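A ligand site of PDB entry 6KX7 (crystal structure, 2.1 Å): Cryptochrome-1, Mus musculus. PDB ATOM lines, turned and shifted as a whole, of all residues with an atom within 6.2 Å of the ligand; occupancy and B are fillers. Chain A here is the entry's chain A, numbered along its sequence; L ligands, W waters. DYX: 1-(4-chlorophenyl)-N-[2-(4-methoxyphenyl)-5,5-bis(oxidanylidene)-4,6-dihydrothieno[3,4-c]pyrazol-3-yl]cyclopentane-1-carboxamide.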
ATOM      1  N   SER A 254       3.980  27.530  14.152  1.00  0.00           N
ATOM      2  CA  SER A 254       3.615  26.275  13.518  1.00  0.00           C
ATOM      3  C   SER A 254       4.691  25.194  13.612  1.00  0.00           C
ATOM      4  O   SER A 254       4.331  24.028  13.839  1.00  0.00           O
ATOM      5  CB  SER A 254       3.191  26.527  12.056  1.00  0.00           C
ATOM      6  OG  SER A 254       4.259  26.869  11.193  1.00  0.00           O
ATOM      7  N   LEU A 257       4.451  23.552  17.089  1.00  0.00           N
ATOM      8  CA  LEU A 257       3.318  22.631  17.233  1.00  0.00           C
ATOM      9  C   LEU A 257       3.618  21.281  16.609  1.00  0.00           C
ATOM     10  O   LEU A 257       3.159  20.250  17.100  1.00  0.00           O
ATOM     11  CB  LEU A 257       2.069  23.248  16.603  1.00  0.00           C
ATOM     12  CG  LEU A 257       1.584  24.516  17.294  1.00  0.00           C
ATOM     13  CD1 LEU A 257       0.482  25.151  16.464  1.00  0.00           C
ATOM     14  CD2 LEU A 257       1.083  24.180  18.687  1.00  0.00           C
ATOM     15  N   GLN A 291      -6.833  26.562  12.099  1.00  0.00           N
ATOM     16  CA  GLN A 291      -5.625  25.811  11.791  1.00  0.00           C
ATOM     17  C   GLN A 291      -5.513  24.564  12.647  1.00  0.00           C
ATOM     18  O   GLN A 291      -5.099  23.501  12.169  1.00  0.00           O
ATOM     19  CB  GLN A 291      -4.402  26.704  11.975  1.00  0.00           C
ATOM     20  CG  GLN A 291      -4.146  27.625  10.794  1.00  0.00           C
ATOM     21  CD  GLN A 291      -3.817  26.845   9.544  1.00  0.00           C
ATOM     22  OE1 GLN A 291      -2.784  26.193   9.467  1.00  0.00           O
ATOM     23  NE2 GLN A 291      -4.708  26.886   8.554  1.00  0.00           N
ATOM     24  N   LEU A 292      -5.887  24.659  13.926  1.00  0.00           N
ATOM     25  CA  LEU A 292      -5.778  23.501  14.814  1.00  0.00           C
ATOM     26  C   LEU A 292      -6.784  22.423  14.432  1.00  0.00           C
ATOM     27  O   LEU A 292      -6.512  21.236  14.598  1.00  0.00           O
ATOM     28  CB  LEU A 292      -5.975  23.939  16.262  1.00  0.00           C
ATOM     29  CG  LEU A 292      -4.858  24.776  16.869  1.00  0.00           C
ATOM     30  CD1 LEU A 292      -5.190  25.150  18.291  1.00  0.00           C
ATOM     31  CD2 LEU A 292      -3.539  24.027  16.804  1.00  0.00           C
ATOM     32  N   TRP A 294      -7.932  21.800  11.325  1.00  0.00           N
ATOM     33  CA  TRP A 294      -7.429  21.127  10.132  1.00  0.00           C
ATOM     34  C   TRP A 294      -6.335  20.146  10.501  1.00  0.00           C
ATOM     35  O   TRP A 294      -6.277  19.029   9.960  1.00  0.00           O
ATOM     36  CB  TRP A 294      -6.903  22.160   9.124  1.00  0.00           C
ATOM     37  CG  TRP A 294      -7.946  22.711   8.188  1.00  0.00           C
ATOM     38  CD1 TRP A 294      -8.448  23.971   8.202  1.00  0.00           C
ATOM     39  CD2 TRP A 294      -8.599  22.017   7.112  1.00  0.00           C
ATOM     40  NE1 TRP A 294      -9.389  24.114   7.206  1.00  0.00           N
ATOM     41  CE2 TRP A 294      -9.491  22.930   6.518  1.00  0.00           C
ATOM     42  CE3 TRP A 294      -8.517  20.730   6.593  1.00  0.00           C
ATOM     43  CZ2 TRP A 294     -10.304  22.599   5.438  1.00  0.00           C
ATOM     44  CZ3 TRP A 294      -9.320  20.393   5.505  1.00  0.00           C
ATOM     45  CH2 TRP A 294     -10.200  21.322   4.947  1.00  0.00           C
ATOM     46  N   ARG A 295      -5.448  20.547  11.401  1.00  0.00           N
ATOM     47  CA  ARG A 295      -4.425  19.660  11.951  1.00  0.00           C
ATOM     48  C   ARG A 295      -5.068  18.405  12.528  1.00  0.00           C
ATOM     49  O   ARG A 295      -4.695  17.277  12.190  1.00  0.00           O
ATOM     50  CB  ARG A 295      -3.646  20.414  13.021  1.00  0.00           C
ATOM     51  CG  ARG A 295      -2.449  19.728  13.589  1.00  0.00           C
ATOM     52  CD  ARG A 295      -1.790  20.670  14.588  1.00  0.00           C
ATOM     53  NE  ARG A 295      -0.688  20.054  15.305  1.00  0.00           N
ATOM     54  CZ  ARG A 295      -0.824  19.404  16.459  1.00  0.00           C
ATOM     55  NH1 ARG A 295      -2.019  19.259  17.008  1.00  0.00           N
ATOM     56  NH2 ARG A 295       0.233  18.886  17.058  1.00  0.00           N
ATOM     57  N   GLU A 296      -6.045  18.603  13.414  1.00  0.00           N
ATOM     58  CA  GLU A 296      -6.713  17.488  14.065  1.00  0.00           C
ATOM     59  C   GLU A 296      -7.420  16.602  13.039  1.00  0.00           C
ATOM     60  O   GLU A 296      -7.408  15.377  13.151  1.00  0.00           O
ATOM     61  CB  GLU A 296      -7.705  18.032  15.085  1.00  0.00           C
ATOM     62  CG  GLU A 296      -8.122  17.041  16.132  1.00  0.00           C
ATOM     63  CD  GLU A 296      -7.169  16.997  17.313  1.00  0.00           C
ATOM     64  OE1 GLU A 296      -6.221  17.817  17.371  1.00  0.00           O
ATOM     65  OE2 GLU A 296      -7.377  16.130  18.189  1.00  0.00           O
ATOM     66  N   PHE A 298      -6.729  15.977   9.797  1.00  0.00           N
ATOM     67  CA  PHE A 298      -5.865  15.124   8.985  1.00  0.00           C
ATOM     68  C   PHE A 298      -5.255  13.999   9.813  1.00  0.00           C
ATOM     69  O   PHE A 298      -5.044  12.887   9.306  1.00  0.00           O
ATOM     70  CB  PHE A 298      -4.765  15.949   8.315  1.00  0.00           C
ATOM     71  CG  PHE A 298      -5.240  16.756   7.138  1.00  0.00           C
ATOM     72  CD1 PHE A 298      -6.204  16.244   6.279  1.00  0.00           C
ATOM     73  CD2 PHE A 298      -4.726  18.016   6.896  1.00  0.00           C
ATOM     74  CE1 PHE A 298      -6.647  16.983   5.204  1.00  0.00           C
ATOM     75  CE2 PHE A 298      -5.169  18.755   5.822  1.00  0.00           C
ATOM     76  CZ  PHE A 298      -6.123  18.246   4.971  1.00  0.00           C
ATOM     77  N   TYR A 299      -4.935  14.276  11.088  1.00  0.00           N
ATOM     78  CA  TYR A 299      -4.504  13.186  11.965  1.00  0.00           C
ATOM     79  C   TYR A 299      -5.593  12.126  12.067  1.00  0.00           C
ATOM     80  O   TYR A 299      -5.320  10.926  11.978  1.00  0.00           O
ATOM     81  CB  TYR A 299      -4.145  13.723  13.348  1.00  0.00           C
ATOM     82  CG  TYR A 299      -2.781  14.387  13.431  1.00  0.00           C
ATOM     83  CD1 TYR A 299      -1.657  13.801  12.858  1.00  0.00           C
ATOM     84  CD2 TYR A 299      -2.620  15.603  14.098  1.00  0.00           C
ATOM     85  CE1 TYR A 299      -0.408  14.406  12.933  1.00  0.00           C
ATOM     86  CE2 TYR A 299      -1.371  16.209  14.195  1.00  0.00           C
ATOM     87  CZ  TYR A 299      -0.270  15.610  13.608  1.00  0.00           C
ATOM     88  OH  TYR A 299       0.958  16.211  13.687  1.00  0.00           O
ATOM     89  N   HIS A 357       1.298  30.071   3.972  1.00  0.00           N
ATOM     90  CA  HIS A 357       0.286  29.168   3.417  1.00  0.00           C
ATOM     91  C   HIS A 357      -0.156  29.590   2.024  1.00  0.00           C
ATOM     92  O   HIS A 357      -0.469  28.726   1.189  1.00  0.00           O
ATOM     93  CB  HIS A 357      -0.915  29.090   4.363  1.00  0.00           C
ATOM     94  CG  HIS A 357      -0.820  27.994   5.378  1.00  0.00           C
ATOM     95  ND1 HIS A 357      -1.931  27.439   5.983  1.00  0.00           N
ATOM     96  CD2 HIS A 357       0.254  27.342   5.889  1.00  0.00           C
ATOM     97  CE1 HIS A 357      -1.540  26.489   6.821  1.00  0.00           C
ATOM     98  NE2 HIS A 357      -0.223  26.418   6.778  1.00  0.00           N
ATOM     99  N   LEU A 358      -0.204  30.891   1.738  1.00  0.00           N
ATOM    100  CA  LEU A 358      -0.530  31.345   0.389  1.00  0.00           C
ATOM    101  C   LEU A 358       0.573  30.994  -0.593  1.00  0.00           C
ATOM    102  O   LEU A 358       0.297  30.756  -1.779  1.00  0.00           O
ATOM    103  CB  LEU A 358      -0.784  32.848   0.359  1.00  0.00           C
ATOM    104  CG  LEU A 358      -2.135  33.312   0.887  1.00  0.00           C
ATOM    105  CD1 LEU A 358      -2.301  34.831   0.797  1.00  0.00           C
ATOM    106  CD2 LEU A 358      -3.261  32.600   0.145  1.00  0.00           C
ATOM    107  N   ARG A 360       2.448  28.281  -0.253  1.00  0.00           N
ATOM    108  CA  ARG A 360       2.278  26.843  -0.459  1.00  0.00           C
ATOM    109  C   ARG A 360       1.223  26.578  -1.524  1.00  0.00           C
ATOM    110  O   ARG A 360       1.423  25.753  -2.424  1.00  0.00           O
ATOM    111  CB  ARG A 360       1.877  26.140   0.864  1.00  0.00           C
ATOM    112  CG  ARG A 360       2.893  26.283   1.987  1.00  0.00           C
ATOM    113  CD  ARG A 360       2.432  25.639   3.327  1.00  0.00           C
ATOM    114  NE  ARG A 360       3.157  26.246   4.446  1.00  0.00           N
ATOM    115  CZ  ARG A 360       3.337  25.699   5.649  1.00  0.00           C
ATOM    116  NH1 ARG A 360       2.851  24.485   5.944  1.00  0.00           N
ATOM    117  NH2 ARG A 360       4.038  26.382   6.557  1.00  0.00           N
ATOM    118  N   HIS A 361       0.084  27.267  -1.426  1.00  0.00           N
ATOM    119  CA  HIS A 361      -0.941  27.198  -2.463  1.00  0.00           C
ATOM    120  C   HIS A 361      -0.336  27.448  -3.839  1.00  0.00           C
ATOM    121  O   HIS A 361      -0.597  26.707  -4.789  1.00  0.00           O
ATOM    122  CB  HIS A 361      -2.046  28.237  -2.180  1.00  0.00           C
ATOM    123  CG  HIS A 361      -3.203  27.702  -1.389  1.00  0.00           C
ATOM    124  ND1 HIS A 361      -4.145  26.844  -1.916  1.00  0.00           N
ATOM    125  CD2 HIS A 361      -3.585  27.950  -0.112  1.00  0.00           C
ATOM    126  CE1 HIS A 361      -5.047  26.574  -0.999  1.00  0.00           C
ATOM    127  NE2 HIS A 361      -4.741  27.229   0.108  1.00  0.00           N
ATOM    128  N   ALA A 362       0.486  28.501  -3.944  1.00  0.00           N
ATOM    129  CA  ALA A 362       1.051  28.877  -5.238  1.00  0.00           C
ATOM    130  C   ALA A 362       1.931  27.766  -5.810  1.00  0.00           C
ATOM    131  O   ALA A 362       1.712  27.321  -6.944  1.00  0.00           O
ATOM    132  CB  ALA A 362       1.853  30.183  -5.102  1.00  0.00           C
ATOM    133  N   ALA A 364       2.207  24.633  -4.940  1.00  0.00           N
ATOM    134  CA  ALA A 364       1.556  23.323  -5.037  1.00  0.00           C
ATOM    135  C   ALA A 364       0.565  23.289  -6.186  1.00  0.00           C
ATOM    136  O   ALA A 364       0.449  22.277  -6.885  1.00  0.00           O
ATOM    137  CB  ALA A 364       0.864  22.984  -3.710  1.00  0.00           C
ATOM    138  N   PHE A 383       8.171  18.413   0.170  1.00  0.00           N
ATOM    139  CA  PHE A 383       7.782  19.144   1.369  1.00  0.00           C
ATOM    140  C   PHE A 383       8.133  18.353   2.625  1.00  0.00           C
ATOM    141  O   PHE A 383       8.572  18.930   3.629  1.00  0.00           O
ATOM    142  CB  PHE A 383       6.285  19.462   1.336  1.00  0.00           C
ATOM    143  CG  PHE A 383       5.951  20.761   0.648  1.00  0.00           C
ATOM    144  CD1 PHE A 383       6.695  21.206  -0.444  1.00  0.00           C
ATOM    145  CD2 PHE A 383       4.871  21.520   1.069  1.00  0.00           C
ATOM    146  CE1 PHE A 383       6.357  22.407  -1.079  1.00  0.00           C
ATOM    147  CE2 PHE A 383       4.535  22.685   0.453  1.00  0.00           C
ATOM    148  CZ  PHE A 383       5.273  23.150  -0.627  1.00  0.00           C
ATOM    149  N   LEU A 387       9.970  21.002   4.841  1.00  0.00           N
ATOM    150  CA  LEU A 387       9.005  21.802   5.596  1.00  0.00           C
ATOM    151  C   LEU A 387       9.051  21.411   7.065  1.00  0.00           C
ATOM    152  O   LEU A 387       9.009  20.227   7.396  1.00  0.00           O
ATOM    153  CB  LEU A 387       7.599  21.599   5.041  1.00  0.00           C
ATOM    154  CG  LEU A 387       6.466  22.540   5.470  1.00  0.00           C
ATOM    155  CD1 LEU A 387       6.791  24.013   5.193  1.00  0.00           C
ATOM    156  CD2 LEU A 387       5.148  22.146   4.797  1.00  0.00           C
ATOM    157  N   ASP A 389       6.810  22.305   9.530  1.00  0.00           N
ATOM    158  CA  ASP A 389       5.607  22.334  10.351  1.00  0.00           C
ATOM    159  C   ASP A 389       4.539  21.341   9.927  1.00  0.00           C
ATOM    160  O   ASP A 389       3.404  21.415  10.412  1.00  0.00           O
ATOM    161  CB  ASP A 389       5.026  23.763  10.404  1.00  0.00           C
ATOM    162  CG  ASP A 389       4.389  24.207   9.091  1.00  0.00           C
ATOM    163  OD1 ASP A 389       4.338  23.433   8.111  1.00  0.00           O
ATOM    164  OD2 ASP A 389       3.921  25.371   9.051  1.00  0.00           O
ATOM    165  N   ALA A 390       4.871  20.380   9.070  1.00  0.00           N
ATOM    166  CA  ALA A 390       3.857  19.469   8.542  1.00  0.00           C
ATOM    167  C   ALA A 390       4.275  18.024   8.792  1.00  0.00           C
ATOM    168  O   ALA A 390       5.172  17.502   8.130  1.00  0.00           O
ATOM    169  CB  ALA A 390       3.630  19.728   7.052  1.00  0.00           C
ATOM    170  N   ILE A 394      -0.469  15.524   7.994  1.00  0.00           N
ATOM    171  CA  ILE A 394      -0.859  16.855   7.531  1.00  0.00           C
ATOM    172  C   ILE A 394      -0.336  17.095   6.119  1.00  0.00           C
ATOM    173  O   ILE A 394      -1.045  17.650   5.274  1.00  0.00           O
ATOM    174  CB  ILE A 394      -0.354  17.934   8.500  1.00  0.00           C
ATOM    175  CG1 ILE A 394      -0.694  17.602   9.950  1.00  0.00           C
ATOM    176  CG2 ILE A 394      -0.777  19.355   8.036  1.00  0.00           C
ATOM    177  CD1 ILE A 394      -2.113  17.204  10.240  1.00  0.00           C
ATOM    178  N   ASN A 395       0.906  16.713   5.861  1.00  0.00           N
ATOM    179  CA  ASN A 395       1.504  16.894   4.545  1.00  0.00           C
ATOM    180  C   ASN A 395       0.719  16.119   3.498  1.00  0.00           C
ATOM    181  O   ASN A 395       0.297  16.681   2.472  1.00  0.00           O
ATOM    182  CB  ASN A 395       2.963  16.452   4.590  1.00  0.00           C
ATOM    183  CG  ASN A 395       3.786  17.016   3.452  1.00  0.00           C
ATOM    184  OD1 ASN A 395       3.391  17.986   2.797  1.00  0.00           O
ATOM    185  ND2 ASN A 395       4.926  16.385   3.186  1.00  0.00           N
ATOM    186  N   ALA A 396       0.475  14.829   3.739  1.00  0.00           N
ATOM    187  CA  ALA A 396      -0.278  14.036   2.779  1.00  0.00           C
ATOM    188  C   ALA A 396      -1.695  14.557   2.621  1.00  0.00           C
ATOM    189  O   ALA A 396      -2.197  14.712   1.500  1.00  0.00           O
ATOM    190  CB  ALA A 396      -0.293  12.565   3.195  1.00  0.00           C
ATOM    191  N   GLY A 397      -2.357  14.841   3.737  1.00  0.00           N
ATOM    192  CA  GLY A 397      -3.705  15.373   3.671  1.00  0.00           C
ATOM    193  C   GLY A 397      -3.768  16.676   2.896  1.00  0.00           C
ATOM    194  O   GLY A 397      -4.691  16.913   2.120  1.00  0.00           O
ATOM    195  N   SER A 398      -2.778  17.537   3.088  1.00  0.00           N
ATOM    196  CA  SER A 398      -2.817  18.844   2.457  1.00  0.00           C
ATOM    197  C   SER A 398      -2.601  18.720   0.953  1.00  0.00           C
ATOM    198  O   SER A 398      -3.278  19.394   0.167  1.00  0.00           O
ATOM    199  CB  SER A 398      -1.777  19.758   3.107  1.00  0.00           C
ATOM    200  OG  SER A 398      -2.189  20.119   4.428  1.00  0.00           O
ATOM    201  N   TRP A 399      -1.720  17.802   0.539  1.00  0.00           N
ATOM    202  CA  TRP A 399      -1.450  17.620  -0.880  1.00  0.00           C
ATOM    203  C   TRP A 399      -2.619  16.946  -1.594  1.00  0.00           C
ATOM    204  O   TRP A 399      -2.933  17.312  -2.738  1.00  0.00           O
ATOM    205  CB  TRP A 399      -0.166  16.814  -1.084  1.00  0.00           C
ATOM    206  CG  TRP A 399       1.047  17.683  -1.012  1.00  0.00           C
ATOM    207  CD1 TRP A 399       1.832  17.888   0.081  1.00  0.00           C
ATOM    208  CD2 TRP A 399       1.599  18.490  -2.059  1.00  0.00           C
ATOM    209  NE1 TRP A 399       2.841  18.767  -0.215  1.00  0.00           N
ATOM    210  CE2 TRP A 399       2.716  19.156  -1.530  1.00  0.00           C
ATOM    211  CE3 TRP A 399       1.257  18.720  -3.400  1.00  0.00           C
ATOM    212  CZ2 TRP A 399       3.503  20.036  -2.279  1.00  0.00           C
ATOM    213  CZ3 TRP A 399       2.034  19.602  -4.149  1.00  0.00           C
ATOM    214  CH2 TRP A 399       3.143  20.243  -3.584  1.00  0.00           C
ATOM    215  N   TRP A 401      -5.685  17.287  -0.679  1.00  0.00           N
ATOM    216  CA  TRP A 401      -6.759  18.262  -0.670  1.00  0.00           C
ATOM    217  C   TRP A 401      -6.598  19.282  -1.796  1.00  0.00           C
ATOM    218  O   TRP A 401      -7.546  19.548  -2.551  1.00  0.00           O
ATOM    219  CB  TRP A 401      -6.822  18.934   0.712  1.00  0.00           C
ATOM    220  CG  TRP A 401      -7.798  20.051   0.809  1.00  0.00           C
ATOM    221  CD1 TRP A 401      -9.148  19.960   1.010  1.00  0.00           C
ATOM    222  CD2 TRP A 401      -7.507  21.454   0.708  1.00  0.00           C
ATOM    223  NE1 TRP A 401      -9.703  21.218   1.039  1.00  0.00           N
ATOM    224  CE2 TRP A 401      -8.720  22.147   0.866  1.00  0.00           C
ATOM    225  CE3 TRP A 401      -6.330  22.181   0.507  1.00  0.00           C
ATOM    226  CZ2 TRP A 401      -8.790  23.546   0.812  1.00  0.00           C
ATOM    227  CZ3 TRP A 401      -6.403  23.568   0.471  1.00  0.00           C
ATOM    228  CH2 TRP A 401      -7.622  24.229   0.612  1.00  0.00           C
ATOM    229  N   LEU A 402      -5.395  19.854  -1.950  1.00  0.00           N
ATOM    230  CA  LEU A 402      -5.210  20.924  -2.934  1.00  0.00           C
ATOM    231  C   LEU A 402      -5.227  20.395  -4.365  1.00  0.00           C
ATOM    232  O   LEU A 402      -5.467  21.164  -5.298  1.00  0.00           O
ATOM    233  CB  LEU A 402      -3.897  21.676  -2.692  1.00  0.00           C
ATOM    234  CG  LEU A 402      -2.624  20.894  -2.986  1.00  0.00           C
ATOM    235  CD1 LEU A 402      -2.054  21.113  -4.413  1.00  0.00           C
ATOM    236  CD2 LEU A 402      -1.596  21.269  -1.944  1.00  0.00           C
HETATM  237  C10 DYX L   1       1.292  21.070   4.725  1.00  0.00           C
HETATM  238  C13 DYX L   1       0.443  22.744   2.651  1.00  0.00           C
HETATM  239  C17 DYX L   1       0.632  23.057   9.963  1.00  0.00           C
HETATM  240  C22 DYX L   1      -4.586  23.496   5.002  1.00  0.00           C
HETATM  241  C24 DYX L   1      -6.814  24.029   4.364  1.00  0.00           C
HETATM  242  C26 DYX L   1      -5.481  22.152   4.949  1.00  0.00           C
HETATM  243  C28 DYX L   1      -3.189  25.038   3.496  1.00  0.00           C
HETATM  244  C01 DYX L   1      -3.477  23.485   6.076  1.00  0.00           C
HETATM  245  C04 DYX L   1      -1.149  22.572   6.809  1.00  0.00           C
HETATM  246  C05 DYX L   1      -1.061  22.846   8.191  1.00  0.00           C
HETATM  247  C06 DYX L   1       0.245  22.807   8.518  1.00  0.00           C
HETATM  248  C09 DYX L   1       0.465  22.165   4.996  1.00  0.00           C
HETATM  249  C11 DYX L   1       1.692  20.804   3.423  1.00  0.00           C
HETATM  250  C12 DYX L   1       1.255  21.634   2.390  1.00  0.00           C
HETATM  251  C14 DYX L   1       0.043  23.015   3.963  1.00  0.00           C
HETATM  252  C16 DYX L   1       0.979  22.142   0.122  1.00  0.00           C
HETATM  253  C19 DYX L   1      -2.020  23.094   9.344  1.00  0.00           C
HETATM  254  C23 DYX L   1      -5.450  24.491   5.203  1.00  0.00           C
HETATM  255  C25 DYX L   1      -6.765  22.668   4.183  1.00  0.00           C
HETATM  256  C27 DYX L   1      -3.817  23.799   3.643  1.00  0.00           C
HETATM  257  C29 DYX L   1      -2.481  25.346   2.332  1.00  0.00           C
HETATM  258  C30 DYX L   1      -2.416  24.387   1.320  1.00  0.00           C
HETATM  259  C31 DYX L   1      -3.036  23.138   1.472  1.00  0.00           C
HETATM  260  C32 DYX L   1      -3.733  22.836   2.632  1.00  0.00           C
HETATM  261  N03 DYX L   1      -2.322  22.566   5.907  1.00  0.00           N
HETATM  262  N07 DYX L   1       0.954  22.539   7.367  1.00  0.00           N
HETATM  263  N08 DYX L   1       0.063  22.438   6.374  1.00  0.00           N
HETATM  264  O02 DYX L   1      -3.573  24.223   6.993  1.00  0.00           O
HETATM  265  O15 DYX L   1       1.652  21.350   1.074  1.00  0.00           O
HETATM  266  O20 DYX L   1      -0.533  23.255  12.122  1.00  0.00           O
HETATM  267  O21 DYX L   1      -1.537  21.414  11.161  1.00  0.00           O
HETATM  268  S18 DYX L   1      -0.952  22.697  10.822  1.00  0.00           S
HETATM  269 CL1  DYX L   1      -1.530  24.725  -0.178  1.00  0.00          CL
HETATM  270  O   HOH W   1       1.300  26.188   8.843  1.00  0.00           O
HETATM  271  O   HOH W   2      -0.867  26.471  11.143  1.00  0.00           O
HETATM  272  O   HOH W   3       2.021  23.098  12.947  1.00  0.00           O
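The side-chain hydroxyl (OG) of Ser 398 lies within hydrogen-bond range of a nitrogen (N03) of the ligand (2.9 Å).
The guanidinium group (NH1) of Arg 360 sits at hydrogen-bond distance from a nitrogen (N07) of the ligand, 3.1 Å away.
The indole nitrogen of Trp 399 lies within hydrogen-bond range of an oxygen (O15) of the ligand, at 3.1 Å.
The side-chain amide oxygen (OE1) of Gln 291 sits close to an oxygen (O02) of the ligand.
The side-chain hydroxyl (OG) of Ser 398 lies within hydrogen-bond range of the backbone carbonyl oxygen (O) of Ile 394.
The guanidinium group of Arg 295 is in hydrogen-bond range of the backbone carbonyl oxygen of Leu 257, 3.2 Å away.
The guanidinium group (NH2) of Arg 360 lies within salt-bridge range of the side-chain carboxylate (OD2) of Asp 389 (2.7 Å).
NE1 of Trp 399 sits close to OD1 of Asn 395 (3.2 Å).
The side-chain carboxylate (OD2) of Asp 389 sits at hydrogen-bond distance from the side-chain hydroxyl (OG) of Ser 254 (2.6 Å).
CD2 of Trp 294 touches C25 of the ligand, 3.5 Å away.
Arg 295 touches the ligand (CB to O21, 3.0 Å).
Phe 298 touches the ligand (CE2 to C26, 3.5 Å).
His 357 touches the ligand.
His 361 touches the ligand (N to CL1, 3.3 Å).
Ala 364 touches the ligand.
Phe 383 touches the ligand.
Leu 387 touches the ligand.
Asp 389 touches the ligand.
CB of Ala 390 touches C10 of the ligand, 3.6 Å away.
CG2 of Ile 394 touches C04 of the ligand (3.5 Å).
Asn 395 touches the ligand.
Trp 401 touches the ligand (CE3 to C32, 3.4 Å).
Leu 402 touches the ligand.
Hydrophobic or aromatic side chains within 4 Å of the ligand: Trp 294, Phe 298, His 357, His 361, Ala 364, Phe 383, Leu 387, Ala 390, Ile 394, Trp 399, Trp 401 and Leu 402.
Within 4 Å of the ligand: Gln 291, Trp 294, Arg 295, Phe 298, His 357, Arg 360, His 361, Ala 364, Phe 383, Leu 387, Asp 389, Ala 390, Ile 394, Asn 395, Ser 398, Trp 399, Trp 401 and Leu 402.
The nearest printed residue that does not touch the ligand is Ser 254 (4.8 Å).
Water W2 bridges the side-chain amide oxygen of Gln 291 (2.6 Å) and an oxygen (O20) of the ligand (3.4 Å).
Water W1 bridges a ring nitrogen (NE2) of His 357 (2.6 Å) and the side-chain carboxylate (OD2) of Asp 389 (2.8 Å).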
